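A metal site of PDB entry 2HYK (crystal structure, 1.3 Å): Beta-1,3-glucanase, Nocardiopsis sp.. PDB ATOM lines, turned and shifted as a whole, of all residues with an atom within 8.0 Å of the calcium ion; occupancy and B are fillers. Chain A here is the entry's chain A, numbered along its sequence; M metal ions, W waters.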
ATOM      1  N   ASP A  13     -30.025   2.299  15.330  1.00  0.00           N
ATOM      2  CA  ASP A  13     -28.954   2.438  16.304  1.00  0.00           C
ATOM      3  C   ASP A  13     -27.767   2.989  15.531  1.00  0.00           C
ATOM      4  O   ASP A  13     -27.287   2.346  14.603  1.00  0.00           O
ATOM      5  CB  ASP A  13     -28.606   1.105  16.977  1.00  0.00           C
ATOM      6  CG  ASP A  13     -27.797   1.304  18.251  1.00  0.00           C
ATOM      7  OD1 ASP A  13     -27.102   2.345  18.372  1.00  0.00           O
ATOM      8  OD2 ASP A  13     -27.846   0.420  19.121  1.00  0.00           O
ATOM      9  N   GLU A  14     -27.356   4.189  15.913  1.00  0.00           N
ATOM     10  CA  GLU A  14     -26.253   4.890  15.252  1.00  0.00           C
ATOM     11  C   GLU A  14     -24.924   4.638  15.952  1.00  0.00           C
ATOM     12  O   GLU A  14     -23.882   5.092  15.490  1.00  0.00           O
ATOM     13  CB  GLU A  14     -26.527   6.399  15.177  1.00  0.00           C
ATOM     14  CG  GLU A  14     -27.859   6.772  14.504  1.00  0.00           C
ATOM     15  CD  GLU A  14     -27.911   6.464  13.009  1.00  0.00           C
ATOM     16  OE1 GLU A  14     -26.865   6.540  12.323  1.00  0.00           O
ATOM     17  OE2 GLU A  14     -29.014   6.165  12.511  1.00  0.00           O
ATOM     18  N   PHE A  15     -24.973   3.915  17.080  1.00  0.00           N
ATOM     19  CA  PHE A  15     -23.774   3.491  17.808  1.00  0.00           C
ATOM     20  C   PHE A  15     -22.906   4.667  18.283  1.00  0.00           C
ATOM     21  O   PHE A  15     -21.677   4.608  18.256  1.00  0.00           O
ATOM     22  CB  PHE A  15     -22.978   2.457  17.004  1.00  0.00           C
ATOM     23  CG  PHE A  15     -23.748   1.202  16.701  1.00  0.00           C
ATOM     24  CD1 PHE A  15     -24.249   0.405  17.743  1.00  0.00           C
ATOM     25  CD2 PHE A  15     -23.997   0.806  15.385  1.00  0.00           C
ATOM     26  CE1 PHE A  15     -24.975  -0.755  17.477  1.00  0.00           C
ATOM     27  CE2 PHE A  15     -24.721  -0.345  15.115  1.00  0.00           C
ATOM     28  CZ  PHE A  15     -25.209  -1.125  16.150  1.00  0.00           C
ATOM     29  N   ASP A  16     -23.587   5.721  18.731  1.00  0.00           N
ATOM     30  CA  ASP A  16     -22.940   6.848  19.390  1.00  0.00           C
ATOM     31  C   ASP A  16     -22.486   6.449  20.782  1.00  0.00           C
ATOM     32  O   ASP A  16     -23.191   5.723  21.505  1.00  0.00           O
ATOM     33  CB  ASP A  16     -23.918   8.030  19.539  1.00  0.00           C
ATOM     34  CG  ASP A  16     -24.566   8.444  18.229  1.00  0.00           C
ATOM     35  OD1 ASP A  16     -23.894   8.398  17.185  1.00  0.00           O
ATOM     36  OD2 ASP A  16     -25.752   8.847  18.255  1.00  0.00           O
ATOM     37  N   GLY A  17     -21.317   6.936  21.180  1.00  0.00           N
ATOM     38  CA  GLY A  17     -20.830   6.738  22.544  1.00  0.00           C
ATOM     39  C   GLY A  17     -19.323   6.535  22.585  1.00  0.00           C
ATOM     40  O   GLY A  17     -18.696   6.275  21.564  1.00  0.00           O
ATOM     41  N   ASP A  55     -16.546   1.911  19.467  1.00  0.00           N
ATOM     42  CA  ASP A  55     -15.156   2.365  19.295  1.00  0.00           C
ATOM     43  C   ASP A  55     -14.900   3.835  19.599  1.00  0.00           C
ATOM     44  O   ASP A  55     -13.759   4.292  19.535  1.00  0.00           O
ATOM     45  CB  ASP A  55     -14.620   1.972  17.907  1.00  0.00           C
ATOM     46  CG  ASP A  55     -15.286   2.717  16.753  1.00  0.00           C
ATOM     47  OD1 ASP A  55     -16.217   3.518  16.982  1.00  0.00           O
ATOM     48  OD2 ASP A  55     -14.855   2.512  15.592  1.00  0.00           O
ATOM     49  N   ASN A  57     -15.871   6.207  17.814  1.00  0.00           N
ATOM     50  CA  ASN A  57     -15.836   6.834  16.499  1.00  0.00           C
ATOM     51  C   ASN A  57     -17.185   6.635  15.789  1.00  0.00           C
ATOM     52  O   ASN A  57     -17.302   6.860  14.574  1.00  0.00           O
ATOM     53  CB  ASN A  57     -14.697   6.235  15.678  1.00  0.00           C
ATOM     54  CG  ASN A  57     -14.400   6.992  14.394  1.00  0.00           C
ATOM     55  OD1 ASN A  57     -13.980   6.399  13.403  1.00  0.00           O
ATOM     56  ND2 ASN A  57     -14.630   8.301  14.411  1.00  0.00           N
ATOM     57  N   GLY A  58     -18.180   6.205  16.544  1.00  0.00           N
ATOM     58  CA  GLY A  58     -19.529   6.013  16.037  1.00  0.00           C
ATOM     59  C   GLY A  58     -19.823   4.644  15.453  1.00  0.00           C
ATOM     60  O   GLY A  58     -20.801   4.477  14.717  1.00  0.00           O
ATOM     61  N   ASN A  59     -18.984   3.651  15.757  1.00  0.00           N
ATOM     62  CA  ASN A  59     -19.194   2.286  15.301  1.00  0.00           C
ATOM     63  C   ASN A  59     -19.346   1.304  16.449  1.00  0.00           C
ATOM     64  O   ASN A  59     -18.676   1.427  17.474  1.00  0.00           O
ATOM     65  CB  ASN A  59     -18.008   1.777  14.454  1.00  0.00           C
ATOM     66  CG  ASN A  59     -17.610   2.734  13.357  1.00  0.00           C
ATOM     67  OD1 ASN A  59     -16.463   3.163  13.283  1.00  0.00           O
ATOM     68  ND2 ASN A  59     -18.551   3.066  12.493  1.00  0.00           N
ATOM     69  N   LEU A  60     -20.210   0.314  16.243  1.00  0.00           N
ATOM     70  CA  LEU A  60     -20.136  -0.936  16.970  1.00  0.00           C
ATOM     71  C   LEU A  60     -18.993  -1.745  16.386  1.00  0.00           C
ATOM     72  O   LEU A  60     -18.841  -1.815  15.160  1.00  0.00           O
ATOM     73  CB  LEU A  60     -21.429  -1.732  16.806  1.00  0.00           C
ATOM     74  CG  LEU A  60     -21.403  -3.185  17.282  1.00  0.00           C
ATOM     75  CD1 LEU A  60     -21.341  -3.254  18.800  1.00  0.00           C
ATOM     76  CD2 LEU A  60     -22.588  -3.949  16.737  1.00  0.00           C
ATOM     77  N   SER A  93     -24.742  -0.343   7.681  1.00  0.00           N
ATOM     78  CA  SER A  93     -23.486   0.059   7.055  1.00  0.00           C
ATOM     79  C   SER A  93     -22.362  -0.641   7.798  1.00  0.00           C
ATOM     80  O   SER A  93     -22.149  -0.388   8.990  1.00  0.00           O
ATOM     81  CB  SER A  93     -23.322   1.568   7.117  1.00  0.00           C
ATOM     82  OG  SER A  93     -22.050   1.928   6.638  1.00  0.00           O
ATOM     83  N   PHE A 168     -16.704   0.687   4.465  1.00  0.00           N
ATOM     84  CA  PHE A 168     -18.091   0.454   4.829  1.00  0.00           C
ATOM     85  C   PHE A 168     -18.966   0.353   3.579  1.00  0.00           C
ATOM     86  O   PHE A 168     -18.800   1.116   2.628  1.00  0.00           O
ATOM     87  CB  PHE A 168     -18.608   1.607   5.700  1.00  0.00           C
ATOM     88  CG  PHE A 168     -18.006   1.625   7.082  1.00  0.00           C
ATOM     89  CD1 PHE A 168     -18.694   1.073   8.155  1.00  0.00           C
ATOM     90  CD2 PHE A 168     -16.754   2.191   7.308  1.00  0.00           C
ATOM     91  CE1 PHE A 168     -18.159   1.083   9.433  1.00  0.00           C
ATOM     92  CE2 PHE A 168     -16.207   2.209   8.583  1.00  0.00           C
ATOM     93  CZ  PHE A 168     -16.906   1.645   9.650  1.00  0.00           C
ATOM     94  N   VAL A 236     -19.614  -1.599  12.484  1.00  0.00           N
ATOM     95  CA  VAL A 236     -20.968  -1.279  12.048  1.00  0.00           C
ATOM     96  C   VAL A 236     -21.254   0.180  12.404  1.00  0.00           C
ATOM     97  O   VAL A 236     -21.308   0.533  13.589  1.00  0.00           O
ATOM     98  CB  VAL A 236     -22.016  -2.222  12.678  1.00  0.00           C
ATOM     99  CG1 VAL A 236     -23.390  -1.974  12.056  1.00  0.00           C
ATOM    100  CG2 VAL A 236     -21.611  -3.693  12.531  1.00  0.00           C
ATOM    101  N   ASP A 237     -21.468   1.020  11.392  1.00  0.00           N
ATOM    102  CA  ASP A 237     -21.703   2.437  11.614  1.00  0.00           C
ATOM    103  C   ASP A 237     -23.133   2.680  12.106  1.00  0.00           C
ATOM    104  O   ASP A 237     -23.367   3.561  12.947  1.00  0.00           O
ATOM    105  CB  ASP A 237     -21.423   3.211  10.312  1.00  0.00           C
ATOM    106  CG  ASP A 237     -21.386   4.725  10.492  1.00  0.00           C
ATOM    107  OD1 ASP A 237     -21.442   5.246  11.630  1.00  0.00           O
ATOM    108  OD2 ASP A 237     -21.296   5.421   9.451  1.00  0.00           O
ATOM    109  N   TYR A 238     -24.079   1.900  11.600  1.00  0.00           N
ATOM    110  CA  TYR A 238     -25.472   2.018  11.992  1.00  0.00           C
ATOM    111  C   TYR A 238     -26.251   0.826  11.491  1.00  0.00           C
ATOM    112  O   TYR A 238     -25.837   0.144  10.546  1.00  0.00           O
ATOM    113  CB  TYR A 238     -26.119   3.313  11.467  1.00  0.00           C
ATOM    114  CG  TYR A 238     -25.959   3.589   9.992  1.00  0.00           C
ATOM    115  CD1 TYR A 238     -26.773   2.964   9.042  1.00  0.00           C
ATOM    116  CD2 TYR A 238     -25.009   4.495   9.550  1.00  0.00           C
ATOM    117  CE1 TYR A 238     -26.619   3.241   7.675  1.00  0.00           C
ATOM    118  CE2 TYR A 238     -24.844   4.782   8.211  1.00  0.00           C
ATOM    119  CZ  TYR A 238     -25.648   4.163   7.281  1.00  0.00           C
ATOM    120  OH  TYR A 238     -25.453   4.462   5.958  1.00  0.00           O
ATOM    121  N   VAL A 239     -27.380   0.597  12.142  1.00  0.00           N
ATOM    122  CA  VAL A 239     -28.439  -0.257  11.645  1.00  0.00           C
ATOM    123  C   VAL A 239     -29.674   0.632  11.580  1.00  0.00           C
ATOM    124  O   VAL A 239     -29.974   1.335  12.548  1.00  0.00           O
ATOM    125  CB  VAL A 239     -28.706  -1.487  12.538  1.00  0.00           C
ATOM    126  CG1 VAL A 239     -29.688  -2.430  11.860  1.00  0.00           C
ATOM    127  CG2 VAL A 239     -27.404  -2.243  12.850  1.00  0.00           C
ATOM    128  N   ARG A 240     -30.361   0.611  10.448  1.00  0.00           N
ATOM    129  CA  ARG A 240     -31.539   1.473  10.211  1.00  0.00           C
ATOM    130  C   ARG A 240     -32.683   0.641   9.651  1.00  0.00           C
ATOM    131  O   ARG A 240     -32.485  -0.215   8.800  1.00  0.00           O
ATOM    132  CB  ARG A 240     -31.201   2.612   9.235  1.00  0.00           C
ATOM    133  CG  ARG A 240     -30.319   3.674   9.865  1.00  0.00           C
ATOM    134  CD  ARG A 240     -29.936   4.770   8.885  1.00  0.00           C
ATOM    135  NE  ARG A 240     -28.997   5.686   9.531  1.00  0.00           N
ATOM    136  CZ  ARG A 240     -28.208   6.524   8.881  1.00  0.00           C
ATOM    137  NH1 ARG A 240     -28.250   6.601   7.553  1.00  0.00           N
ATOM    138  NH2 ARG A 240     -27.365   7.298   9.564  1.00  0.00           N
HETATM  139 CA    CA M   1     -22.519   5.661  13.660  1.00  0.00          CA
HETATM  140  O   HOH W   1     -22.519   7.492  15.321  1.00  0.00           O
HETATM  141  O   HOH W   2     -21.086   7.554  13.007  1.00  0.00           O
HETATM  142  O   HOH W   3     -24.189   6.765  12.431  1.00  0.00           O
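The backbone NH (N) of Gly 58 lies within hydrogen-bond range of the side-chain carboxylate (OD1) of Asp 55 (3.4 Å). N of Asp 237 lies within hydrogen-bond range of O of Ser 93. OE1 of Glu 14 lies within salt-bridge range of NH2 of Arg 240, 2.9 Å away.
Three residues have an atom within 4 Å of the calcium ion: Glu 14, Gly 58 and Asp 237.
The calcium ion is bound by OD1 of Asp 237 (2.3 Å), O of Gly 58 (2.3 Å), water W3 (2.3 Å), O of Glu 14 (2.4 Å), O of Asp 237 (2.4 Å), water W2 (2.5 Å) and water W1 (2.5 Å).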
